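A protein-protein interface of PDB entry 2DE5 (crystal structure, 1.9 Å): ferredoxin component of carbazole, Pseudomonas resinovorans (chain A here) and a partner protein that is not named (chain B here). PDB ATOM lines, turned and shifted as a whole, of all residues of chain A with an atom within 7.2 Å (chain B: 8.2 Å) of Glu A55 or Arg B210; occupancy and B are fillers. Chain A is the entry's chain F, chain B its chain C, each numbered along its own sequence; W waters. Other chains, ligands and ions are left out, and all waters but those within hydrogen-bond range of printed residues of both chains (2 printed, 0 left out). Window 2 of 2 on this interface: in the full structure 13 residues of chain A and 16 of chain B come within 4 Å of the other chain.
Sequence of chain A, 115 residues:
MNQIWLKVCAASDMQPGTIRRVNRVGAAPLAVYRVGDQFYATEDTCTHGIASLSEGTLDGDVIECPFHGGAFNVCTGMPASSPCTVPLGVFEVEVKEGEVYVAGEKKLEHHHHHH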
ATOM      1  N   ILE A  19     -15.823   3.921 -16.051  1.00  0.00           N
ATOM      2  CA  ILE A  19     -17.227   3.757 -16.380  1.00  0.00           C
ATOM      3  C   ILE A  19     -17.970   5.068 -16.201  1.00  0.00           C
ATOM      4  O   ILE A  19     -17.706   5.825 -15.265  1.00  0.00           O
ATOM      5  CB  ILE A  19     -17.875   2.698 -15.471  1.00  0.00           C
ATOM      6  CG1 ILE A  19     -16.932   1.500 -15.327  1.00  0.00           C
ATOM      7  CG2 ILE A  19     -19.210   2.249 -16.060  1.00  0.00           C
ATOM      8  CD1 ILE A  19     -17.346   0.519 -14.260  1.00  0.00           C
ATOM      9  N   ARG A  21     -21.967   6.780 -16.248  1.00  0.00           N
ATOM     10  CA  ARG A  21     -23.396   6.526 -16.227  1.00  0.00           C
ATOM     11  C   ARG A  21     -24.091   7.494 -17.180  1.00  0.00           C
ATOM     12  O   ARG A  21     -23.800   8.692 -17.183  1.00  0.00           O
ATOM     13  CB  ARG A  21     -23.951   6.696 -14.811  1.00  0.00           C
ATOM     14  CG  ARG A  21     -25.459   6.523 -14.725  1.00  0.00           C
ATOM     15  CD  ARG A  21     -25.940   6.556 -13.285  1.00  0.00           C
ATOM     16  NE  ARG A  21     -27.398   6.509 -13.205  1.00  0.00           N
ATOM     17  CZ  ARG A  21     -28.078   6.337 -12.077  1.00  0.00           C
ATOM     18  NH1 ARG A  21     -27.431   6.194 -10.927  1.00  0.00           N
ATOM     19  NH2 ARG A  21     -29.402   6.307 -12.098  1.00  0.00           N
ATOM     20  N   ALA A  31     -24.832   2.320 -18.807  1.00  0.00           N
ATOM     21  CA  ALA A  31     -23.461   2.414 -18.344  1.00  0.00           C
ATOM     22  C   ALA A  31     -22.569   2.251 -19.561  1.00  0.00           C
ATOM     23  O   ALA A  31     -22.737   1.315 -20.342  1.00  0.00           O
ATOM     24  CB  ALA A  31     -23.165   1.317 -17.318  1.00  0.00           C
ATOM     25  N   ASP A  44     -27.453   0.218 -16.847  1.00  0.00           N
ATOM     26  CA  ASP A  44     -26.632   0.539 -15.683  1.00  0.00           C
ATOM     27  C   ASP A  44     -27.030  -0.215 -14.418  1.00  0.00           C
ATOM     28  O   ASP A  44     -26.196  -0.454 -13.542  1.00  0.00           O
ATOM     29  CB  ASP A  44     -26.680   2.038 -15.386  1.00  0.00           C
ATOM     30  CG  ASP A  44     -25.849   2.415 -14.166  1.00  0.00           C
ATOM     31  OD1 ASP A  44     -24.626   2.153 -14.173  1.00  0.00           O
ATOM     32  OD2 ASP A  44     -26.416   2.967 -13.202  1.00  0.00           O
ATOM     33  N   ILE A  50     -30.610  -3.302  -7.186  1.00  0.00           N
ATOM     34  CA  ILE A  50     -30.756  -1.891  -7.533  1.00  0.00           C
ATOM     35  C   ILE A  50     -29.403  -1.185  -7.623  1.00  0.00           C
ATOM     36  O   ILE A  50     -29.343   0.041  -7.695  1.00  0.00           O
ATOM     37  CB  ILE A  50     -31.614  -1.133  -6.489  1.00  0.00           C
ATOM     38  CG1 ILE A  50     -30.971  -1.232  -5.104  1.00  0.00           C
ATOM     39  CG2 ILE A  50     -33.022  -1.702  -6.459  1.00  0.00           C
ATOM     40  CD1 ILE A  50     -31.688  -0.412  -4.032  1.00  0.00           C
ATOM     41  N   ALA A  51     -28.323  -1.960  -7.612  1.00  0.00           N
ATOM     42  CA  ALA A  51     -26.978  -1.397  -7.678  1.00  0.00           C
ATOM     43  C   ALA A  51     -26.700  -0.751  -9.027  1.00  0.00           C
ATOM     44  O   ALA A  51     -27.256  -1.149 -10.052  1.00  0.00           O
ATOM     45  CB  ALA A  51     -25.934  -2.480  -7.413  1.00  0.00           C
ATOM     46  N   SER A  52     -25.824   0.247  -9.013  1.00  0.00           N
ATOM     47  CA  SER A  52     -25.434   0.936 -10.238  1.00  0.00           C
ATOM     48  C   SER A  52     -24.105   0.341 -10.681  1.00  0.00           C
ATOM     49  O   SER A  52     -23.091   0.503  -9.998  1.00  0.00           O
ATOM     50  CB  SER A  52     -25.268   2.434  -9.969  1.00  0.00           C
ATOM     51  OG  SER A  52     -24.861   3.110 -11.143  1.00  0.00           O
ATOM     52  N   LEU A  53     -24.107  -0.355 -11.813  1.00  0.00           N
ATOM     53  CA  LEU A  53     -22.884  -0.971 -12.311  1.00  0.00           C
ATOM     54  C   LEU A  53     -21.798   0.065 -12.599  1.00  0.00           C
ATOM     55  O   LEU A  53     -20.607  -0.260 -12.584  1.00  0.00           O
ATOM     56  CB  LEU A  53     -23.176  -1.800 -13.564  1.00  0.00           C
ATOM     57  CG  LEU A  53     -24.115  -2.995 -13.327  1.00  0.00           C
ATOM     58  CD1 LEU A  53     -24.429  -3.681 -14.646  1.00  0.00           C
ATOM     59  CD2 LEU A  53     -23.460  -3.973 -12.348  1.00  0.00           C
ATOM     60  N   SER A  54     -22.210   1.307 -12.853  1.00  0.00           N
ATOM     61  CA  SER A  54     -21.255   2.382 -13.126  1.00  0.00           C
ATOM     62  C   SER A  54     -20.457   2.716 -11.863  1.00  0.00           C
ATOM     63  O   SER A  54     -19.484   3.470 -11.908  1.00  0.00           O
ATOM     64  CB  SER A  54     -21.986   3.634 -13.627  1.00  0.00           C
ATOM     65  OG  SER A  54     -22.819   4.174 -12.617  1.00  0.00           O
ATOM     66  N   GLU A  55     -20.876   2.155 -10.733  1.00  0.00           N
ATOM     67  CA  GLU A  55     -20.176   2.380  -9.472  1.00  0.00           C
ATOM     68  C   GLU A  55     -19.493   1.072  -9.076  1.00  0.00           C
ATOM     69  O   GLU A  55     -19.127   0.867  -7.917  1.00  0.00           O
ATOM     70  CB  GLU A  55     -21.158   2.818  -8.381  1.00  0.00           C
ATOM     71  CG  GLU A  55     -21.930   4.090  -8.709  1.00  0.00           C
ATOM     72  CD  GLU A  55     -22.858   4.522  -7.584  1.00  0.00           C
ATOM     73  OE1 GLU A  55     -23.658   3.683  -7.119  1.00  0.00           O
ATOM     74  OE2 GLU A  55     -22.794   5.697  -7.164  1.00  0.00           O
ATOM     75  N   GLY A  56     -19.321   0.198 -10.064  1.00  0.00           N
ATOM     76  CA  GLY A  56     -18.693  -1.088  -9.830  1.00  0.00           C
ATOM     77  C   GLY A  56     -17.231  -1.142 -10.227  1.00  0.00           C
ATOM     78  O   GLY A  56     -16.599  -0.113 -10.456  1.00  0.00           O
ATOM     79  N   THR A  57     -16.698  -2.355 -10.320  1.00  0.00           N
ATOM     80  CA  THR A  57     -15.298  -2.560 -10.667  1.00  0.00           C
ATOM     81  C   THR A  57     -15.149  -3.268 -12.000  1.00  0.00           C
ATOM     82  O   THR A  57     -15.650  -4.375 -12.191  1.00  0.00           O
ATOM     83  CB  THR A  57     -14.579  -3.400  -9.587  1.00  0.00           C
ATOM     84  OG1 THR A  57     -14.706  -2.751  -8.316  1.00  0.00           O
ATOM     85  CG2 THR A  57     -13.103  -3.558  -9.924  1.00  0.00           C
ATOM     86  N   ILE A  63     -17.601  -6.454 -15.734  1.00  0.00           N
ATOM     87  CA  ILE A  63     -17.952  -5.456 -14.737  1.00  0.00           C
ATOM     88  C   ILE A  63     -18.433  -6.171 -13.471  1.00  0.00           C
ATOM     89  O   ILE A  63     -19.283  -7.060 -13.534  1.00  0.00           O
ATOM     90  CB  ILE A  63     -19.059  -4.505 -15.264  1.00  0.00           C
ATOM     91  CG1 ILE A  63     -19.374  -3.444 -14.208  1.00  0.00           C
ATOM     92  CG2 ILE A  63     -20.301  -5.294 -15.643  1.00  0.00           C
ATOM     93  CD1 ILE A  63     -18.179  -2.596 -13.841  1.00  0.00           C
ATOM     94  N   GLU A  64     -17.863  -5.798 -12.329  1.00  0.00           N
ATOM     95  CA  GLU A  64     -18.237  -6.398 -11.053  1.00  0.00           C
ATOM     96  C   GLU A  64     -19.166  -5.452 -10.300  1.00  0.00           C
ATOM     97  O   GLU A  64     -18.831  -4.290 -10.068  1.00  0.00           O
ATOM     98  CB  GLU A  64     -16.993  -6.671 -10.205  1.00  0.00           C
ATOM     99  CG  GLU A  64     -17.269  -7.517  -8.968  1.00  0.00           C
ATOM    100  CD  GLU A  64     -16.056  -7.664  -8.065  1.00  0.00           C
ATOM    101  OE1 GLU A  64     -14.947  -7.925  -8.587  1.00  0.00           O
ATOM    102  OE2 GLU A  64     -16.215  -7.529  -6.832  1.00  0.00           O
ATOM    103  N   CYS A  65     -20.336  -5.953  -9.921  1.00  0.00           N
ATOM    104  CA  CYS A  65     -21.309  -5.144  -9.196  1.00  0.00           C
ATOM    105  C   CYS A  65     -20.801  -4.784  -7.795  1.00  0.00           C
ATOM    106  O   CYS A  65     -20.280  -5.638  -7.078  1.00  0.00           O
ATOM    107  CB  CYS A  65     -22.630  -5.903  -9.087  1.00  0.00           C
ATOM    108  SG  CYS A  65     -23.854  -5.015  -8.133  1.00  0.00           S
ATOM    109  N   PRO A  66     -20.969  -3.515  -7.382  1.00  0.00           N
ATOM    110  CA  PRO A  66     -20.529  -3.020  -6.072  1.00  0.00           C
ATOM    111  C   PRO A  66     -21.289  -3.556  -4.859  1.00  0.00           C
ATOM    112  O   PRO A  66     -20.805  -3.458  -3.728  1.00  0.00           O
ATOM    113  CB  PRO A  66     -20.689  -1.511  -6.212  1.00  0.00           C
ATOM    114  CG  PRO A  66     -21.900  -1.397  -7.075  1.00  0.00           C
ATOM    115  CD  PRO A  66     -21.615  -2.434  -8.150  1.00  0.00           C
ATOM    116  N   PHE A  67     -22.473  -4.113  -5.095  1.00  0.00           N
ATOM    117  CA  PHE A  67     -23.308  -4.643  -4.017  1.00  0.00           C
ATOM    118  C   PHE A  67     -22.945  -6.032  -3.507  1.00  0.00           C
ATOM    119  O   PHE A  67     -22.556  -6.195  -2.346  1.00  0.00           O
ATOM    120  CB  PHE A  67     -24.780  -4.662  -4.458  1.00  0.00           C
ATOM    121  CG  PHE A  67     -25.536  -3.400  -4.137  1.00  0.00           C
ATOM    122  CD1 PHE A  67     -24.900  -2.161  -4.143  1.00  0.00           C
ATOM    123  CD2 PHE A  67     -26.909  -3.448  -3.899  1.00  0.00           C
ATOM    124  CE1 PHE A  67     -25.623  -0.987  -3.921  1.00  0.00           C
ATOM    125  CE2 PHE A  67     -27.641  -2.279  -3.678  1.00  0.00           C
ATOM    126  CZ  PHE A  67     -26.998  -1.047  -3.691  1.00  0.00           C
ATOM    127  N   LYS B  13     -18.339  -5.231  -0.891  1.00  0.00           N
ATOM    128  CA  LYS B  13     -17.435  -4.086  -0.784  1.00  0.00           C
ATOM    129  C   LYS B  13     -18.075  -2.812  -0.236  1.00  0.00           C
ATOM    130  O   LYS B  13     -17.388  -1.961   0.329  1.00  0.00           O
ATOM    131  CB  LYS B  13     -16.826  -3.772  -2.157  1.00  0.00           C
ATOM    132  CG  LYS B  13     -15.933  -4.864  -2.727  1.00  0.00           C
ATOM    133  CD  LYS B  13     -15.324  -4.427  -4.054  1.00  0.00           C
ATOM    134  CE  LYS B  13     -14.310  -5.436  -4.570  1.00  0.00           C
ATOM    135  NZ  LYS B  13     -14.915  -6.780  -4.774  1.00  0.00           N
ATOM    136  N   GLY B 207     -39.903   8.417  -5.598  1.00  0.00           N
ATOM    137  CA  GLY B 207     -39.829   9.536  -6.520  1.00  0.00           C
ATOM    138  C   GLY B 207     -38.468  10.192  -6.380  1.00  0.00           C
ATOM    139  O   GLY B 207     -37.786   9.981  -5.380  1.00  0.00           O
ATOM    140  N   GLY B 208     -38.063  10.976  -7.375  1.00  0.00           N
ATOM    141  CA  GLY B 208     -36.771  11.641  -7.308  1.00  0.00           C
ATOM    142  C   GLY B 208     -35.595  10.695  -7.452  1.00  0.00           C
ATOM    143  O   GLY B 208     -35.776   9.513  -7.740  1.00  0.00           O
ATOM    144  N   ASP B 209     -34.383  11.208  -7.248  1.00  0.00           N
ATOM    145  CA  ASP B 209     -33.177  10.393  -7.367  1.00  0.00           C
ATOM    146  C   ASP B 209     -32.824   9.664  -6.074  1.00  0.00           C
ATOM    147  O   ASP B 209     -33.511   9.796  -5.062  1.00  0.00           O
ATOM    148  CB  ASP B 209     -31.988  11.256  -7.794  1.00  0.00           C
ATOM    149  CG  ASP B 209     -31.750  12.423  -6.857  1.00  0.00           C
ATOM    150  OD1 ASP B 209     -31.889  12.243  -5.629  1.00  0.00           O
ATOM    151  OD2 ASP B 209     -31.409  13.521  -7.348  1.00  0.00           O
ATOM    152  N   ARG B 210     -31.734   8.907  -6.121  1.00  0.00           N
ATOM    153  CA  ARG B 210     -31.273   8.134  -4.975  1.00  0.00           C
ATOM    154  C   ARG B 210     -31.016   8.974  -3.731  1.00  0.00           C
ATOM    155  O   ARG B 210     -31.607   8.732  -2.676  1.00  0.00           O
ATOM    156  CB  ARG B 210     -29.994   7.376  -5.333  1.00  0.00           C
ATOM    157  CG  ARG B 210     -29.408   6.597  -4.166  1.00  0.00           C
ATOM    158  CD  ARG B 210     -27.909   6.411  -4.315  1.00  0.00           C
ATOM    159  NE  ARG B 210     -27.567   5.598  -5.475  1.00  0.00           N
ATOM    160  CZ  ARG B 210     -26.324   5.299  -5.838  1.00  0.00           C
ATOM    161  NH1 ARG B 210     -25.295   5.750  -5.129  1.00  0.00           N
ATOM    162  NH2 ARG B 210     -26.107   4.544  -6.909  1.00  0.00           N
ATOM    163  N   LYS B 211     -30.133   9.962  -3.855  1.00  0.00           N
ATOM    164  CA  LYS B 211     -29.787  10.809  -2.721  1.00  0.00           C
ATOM    165  C   LYS B 211     -30.993  11.410  -2.002  1.00  0.00           C
ATOM    166  O   LYS B 211     -30.933  11.670  -0.801  1.00  0.00           O
ATOM    167  CB  LYS B 211     -28.836  11.926  -3.158  1.00  0.00           C
ATOM    168  CG  LYS B 211     -28.249  12.701  -1.986  1.00  0.00           C
ATOM    169  CD  LYS B 211     -27.213  13.721  -2.434  1.00  0.00           C
ATOM    170  CE  LYS B 211     -26.636  14.472  -1.237  1.00  0.00           C
ATOM    171  NZ  LYS B 211     -25.671  15.533  -1.646  1.00  0.00           N
ATOM    172  N   GLN B 212     -32.086  11.627  -2.729  1.00  0.00           N
ATOM    173  CA  GLN B 212     -33.295  12.198  -2.134  1.00  0.00           C
ATOM    174  C   GLN B 212     -34.081  11.203  -1.280  1.00  0.00           C
ATOM    175  O   GLN B 212     -34.954  11.598  -0.509  1.00  0.00           O
ATOM    176  CB  GLN B 212     -34.226  12.733  -3.224  1.00  0.00           C
ATOM    177  CG  GLN B 212     -33.728  13.980  -3.934  1.00  0.00           C
ATOM    178  CD  GLN B 212     -34.611  14.359  -5.109  1.00  0.00           C
ATOM    179  OE1 GLN B 212     -34.593  13.705  -6.153  1.00  0.00           O
ATOM    180  NE2 GLN B 212     -35.402  15.411  -4.936  1.00  0.00           N
ATOM    181  N   GLN B 213     -33.778   9.916  -1.417  1.00  0.00           N
ATOM    182  CA  GLN B 213     -34.501   8.896  -0.660  1.00  0.00           C
ATOM    183  C   GLN B 213     -34.170   8.909   0.829  1.00  0.00           C
ATOM    184  O   GLN B 213     -34.939   8.403   1.651  1.00  0.00           O
ATOM    185  CB  GLN B 213     -34.215   7.507  -1.241  1.00  0.00           C
ATOM    186  CG  GLN B 213     -34.475   7.393  -2.738  1.00  0.00           C
ATOM    187  CD  GLN B 213     -35.846   7.910  -3.133  1.00  0.00           C
ATOM    188  OE1 GLN B 213     -36.868   7.457  -2.615  1.00  0.00           O
ATOM    189  NE2 GLN B 213     -35.873   8.865  -4.054  1.00  0.00           N
ATOM    190  N   THR B 214     -33.027   9.492   1.178  1.00  0.00           N
ATOM    191  CA  THR B 214     -32.622   9.556   2.575  1.00  0.00           C
ATOM    192  C   THR B 214     -31.830  10.813   2.876  1.00  0.00           C
ATOM    193  O   THR B 214     -31.478  11.571   1.976  1.00  0.00           O
ATOM    194  CB  THR B 214     -31.700   8.383   2.958  1.00  0.00           C
ATOM    195  OG1 THR B 214     -30.502   8.448   2.171  1.00  0.00           O
ATOM    196  CG2 THR B 214     -32.386   7.052   2.723  1.00  0.00           C
ATOM    197  N   ARG B 215     -31.562  11.014   4.162  1.00  0.00           N
ATOM    198  CA  ARG B 215     -30.743  12.123   4.616  1.00  0.00           C
ATOM    199  C   ARG B 215     -29.766  11.516   5.613  1.00  0.00           C
ATOM    200  O   ARG B 215     -30.147  11.117   6.716  1.00  0.00           O
ATOM    201  CB  ARG B 215     -31.568  13.216   5.292  1.00  0.00           C
ATOM    202  CG  ARG B 215     -30.698  14.399   5.729  1.00  0.00           C
ATOM    203  CD  ARG B 215     -31.511  15.622   6.119  1.00  0.00           C
ATOM    204  NE  ARG B 215     -32.252  15.430   7.361  1.00  0.00           N
ATOM    205  CZ  ARG B 215     -33.575  15.519   7.462  1.00  0.00           C
ATOM    206  NH1 ARG B 215     -34.306  15.795   6.390  1.00  0.00           N
ATOM    207  NH2 ARG B 215     -34.167  15.332   8.636  1.00  0.00           N
ATOM    208  N   LEU B 230     -36.645   9.300   3.856  1.00  0.00           N
ATOM    209  CA  LEU B 230     -37.429  10.354   3.214  1.00  0.00           C
ATOM    210  C   LEU B 230     -38.182   9.879   1.974  1.00  0.00           C
ATOM    211  O   LEU B 230     -38.506  10.681   1.094  1.00  0.00           O
ATOM    212  CB  LEU B 230     -36.507  11.507   2.816  1.00  0.00           C
ATOM    213  CG  LEU B 230     -35.588  12.099   3.889  1.00  0.00           C
ATOM    214  CD1 LEU B 230     -34.751  13.207   3.260  1.00  0.00           C
ATOM    215  CD2 LEU B 230     -36.408  12.644   5.050  1.00  0.00           C
ATOM    216  N   HIS B 234     -40.977  12.485  -2.000  1.00  0.00           N
ATOM    217  CA  HIS B 234     -41.185  12.593  -3.438  1.00  0.00           C
ATOM    218  C   HIS B 234     -41.931  11.371  -3.951  1.00  0.00           C
ATOM    219  O   HIS B 234     -42.260  11.277  -5.134  1.00  0.00           O
ATOM    220  CB  HIS B 234     -39.841  12.702  -4.158  1.00  0.00           C
ATOM    221  CG  HIS B 234     -38.994  13.842  -3.688  1.00  0.00           C
ATOM    222  ND1 HIS B 234     -39.411  15.154  -3.751  1.00  0.00           N
ATOM    223  CD2 HIS B 234     -37.753  13.866  -3.147  1.00  0.00           C
ATOM    224  CE1 HIS B 234     -38.463  15.938  -3.269  1.00  0.00           C
ATOM    225  NE2 HIS B 234     -37.446  15.181  -2.896  1.00  0.00           N
ATOM    226  N   GLU B 357     -36.293  -0.959  -5.088  1.00  0.00           N
ATOM    227  CA  GLU B 357     -36.188   0.465  -4.768  1.00  0.00           C
ATOM    228  C   GLU B 357     -36.173   0.969  -3.329  1.00  0.00           C
ATOM    229  O   GLU B 357     -35.248   1.690  -2.945  1.00  0.00           O
ATOM    230  CB  GLU B 357     -37.227   1.250  -5.574  1.00  0.00           C
ATOM    231  CG  GLU B 357     -36.947   1.275  -7.075  1.00  0.00           C
ATOM    232  CD  GLU B 357     -37.361  -0.007  -7.781  1.00  0.00           C
ATOM    233  OE1 GLU B 357     -37.920  -0.902  -7.117  1.00  0.00           O
ATOM    234  OE2 GLU B 357     -37.139  -0.116  -9.006  1.00  0.00           O
ATOM    235  N   GLU B 360     -33.227   1.236  -0.684  1.00  0.00           N
ATOM    236  CA  GLU B 360     -32.203   2.264  -0.761  1.00  0.00           C
ATOM    237  C   GLU B 360     -31.915   2.774   0.661  1.00  0.00           C
ATOM    238  O   GLU B 360     -30.778   3.114   0.995  1.00  0.00           O
ATOM    239  CB  GLU B 360     -32.679   3.411  -1.658  1.00  0.00           C
ATOM    240  CG  GLU B 360     -31.545   4.239  -2.251  1.00  0.00           C
ATOM    241  CD  GLU B 360     -30.612   3.418  -3.136  1.00  0.00           C
ATOM    242  OE1 GLU B 360     -31.051   2.943  -4.210  1.00  0.00           O
ATOM    243  OE2 GLU B 360     -29.436   3.244  -2.756  1.00  0.00           O
ATOM    244  N   ALA B 361     -32.950   2.813   1.499  1.00  0.00           N
ATOM    245  CA  ALA B 361     -32.796   3.267   2.879  1.00  0.00           C
ATOM    246  C   ALA B 361     -31.918   2.302   3.669  1.00  0.00           C
ATOM    247  O   ALA B 361     -31.044   2.719   4.430  1.00  0.00           O
ATOM    248  CB  ALA B 361     -34.163   3.396   3.547  1.00  0.00           C
ATOM    249  N   VAL B 363     -29.674   0.266   2.464  1.00  0.00           N
ATOM    250  CA  VAL B 363     -28.326   0.380   1.917  1.00  0.00           C
ATOM    251  C   VAL B 363     -27.610   1.585   2.524  1.00  0.00           C
ATOM    252  O   VAL B 363     -26.426   1.517   2.851  1.00  0.00           O
ATOM    253  CB  VAL B 363     -28.365   0.530   0.373  1.00  0.00           C
ATOM    254  CG1 VAL B 363     -26.989   0.916  -0.157  1.00  0.00           C
ATOM    255  CG2 VAL B 363     -28.824  -0.781  -0.257  1.00  0.00           C
ATOM    256  N   ALA B 364     -28.334   2.689   2.673  1.00  0.00           N
ATOM    257  CA  ALA B 364     -27.763   3.897   3.262  1.00  0.00           C
ATOM    258  C   ALA B 364     -27.315   3.599   4.697  1.00  0.00           C
ATOM    259  O   ALA B 364     -26.227   4.001   5.121  1.00  0.00           O
ATOM    260  CB  ALA B 364     -28.791   5.012   3.253  1.00  0.00           C
ATOM    261  N   LYS B 367     -24.188   1.433   4.818  1.00  0.00           N
ATOM    262  CA  LYS B 367     -23.000   2.226   4.521  1.00  0.00           C
ATOM    263  C   LYS B 367     -22.619   3.122   5.695  1.00  0.00           C
ATOM    264  O   LYS B 367     -21.439   3.257   6.023  1.00  0.00           O
ATOM    265  CB  LYS B 367     -23.224   3.084   3.274  1.00  0.00           C
ATOM    266  CG  LYS B 367     -23.236   2.305   1.968  1.00  0.00           C
ATOM    267  CD  LYS B 367     -23.546   3.224   0.783  1.00  0.00           C
ATOM    268  CE  LYS B 367     -23.306   2.524  -0.543  1.00  0.00           C
ATOM    269  NZ  LYS B 367     -24.022   1.225  -0.623  1.00  0.00           N
HETATM  270  O   HOH W   1     -28.514   6.009  -8.300  1.00  0.00           O
HETATM  271  O   HOH W   2     -18.290  -6.536  -5.130  1.00  0.00           O
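The side-chain amino group of Lys B13 is in salt-bridge range of the side-chain carboxylate of Glu A64. The side-chain carboxylate (OE1) of Glu A55 lies within salt-bridge range of the guanidinium group (NH2) of Arg B210.
The side-chain carboxylate of Asp A44 sits at hydrogen-bond distance from the side-chain hydroxyl of Ser A52. The side-chain hydroxyl (OG) of Ser A54 lies within hydrogen-bond range of the side-chain hydroxyl (OG) of Ser A52, at 2.7 Å. The backbone NH (N) of Glu A64 sits at hydrogen-bond distance from the backbone carbonyl oxygen (O) of Thr A57 (2.6 Å). The backbone NH of Phe A67 sits close to the side-chain sulfur of Cys A65 (3.5 Å).
CG2 of Ile A50 touches N of Glu B357, 3.6 Å away. Glu B360 touches Ile A50 (OE1 to CD1, 3.4 Å). CB of Ser A52 touches NH2 of Arg B210 (3.8 Å). Phe A67 touches Val B363 (CZ to CG2, 3.9 Å).
Ile A19 touches none of the printed residues of chain B. No residue of chain B comes within 4 Å of Ser A54. Glu A55 touches just one residue of chain B: Arg B210 (2.6 Å). Printed residues of chain B within 4 Å of Phe A67: Val B363. Of the printed residues of chain A, Lys B13 touches Glu A64. Arg B210 touches just these residues of chain A: Ser A52 (3.8 Å) and Glu A55 (2.6 Å). His B234 touches none of the printed residues of chain A. Of the printed residues of chain A, Glu B357 touches Ile A50. Printed residues of chain A within 4 Å of Glu B360: Ile A50 (3.4 Å). Printed residues of chain A within 4 Å of Val B363: Phe A67. The nearest residue of chain A that does not touch Arg B210 is Arg A21 (4.5 Å).
Of the 18 printed residues of chain B, 5 touch a printed residue of chain A. Printed residues of chain B that touch a printed residue of chain A: Lys B13, Arg B210, Glu B357, Glu B360 and Val B363. Hydrophobic or aromatic side chains of chain B within 4 Å of the printed part of chain A: Val B363. Along chain B the printed residues that touch a printed residue of chain A span positions 13 to 363. Hydrophobic or aromatic side chains of chain A that line the printed part of chain B: Ile A50 and Phe A67.
Water W1 lies within hydrogen-bond range of NH1 of Arg A21 and NE of Arg B210. Water W2 lies within hydrogen-bond range of OE2 of Glu A64 (2.9 Å), O of Cys A65 (2.9 Å) and NZ of Lys B13 (3.4 Å).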
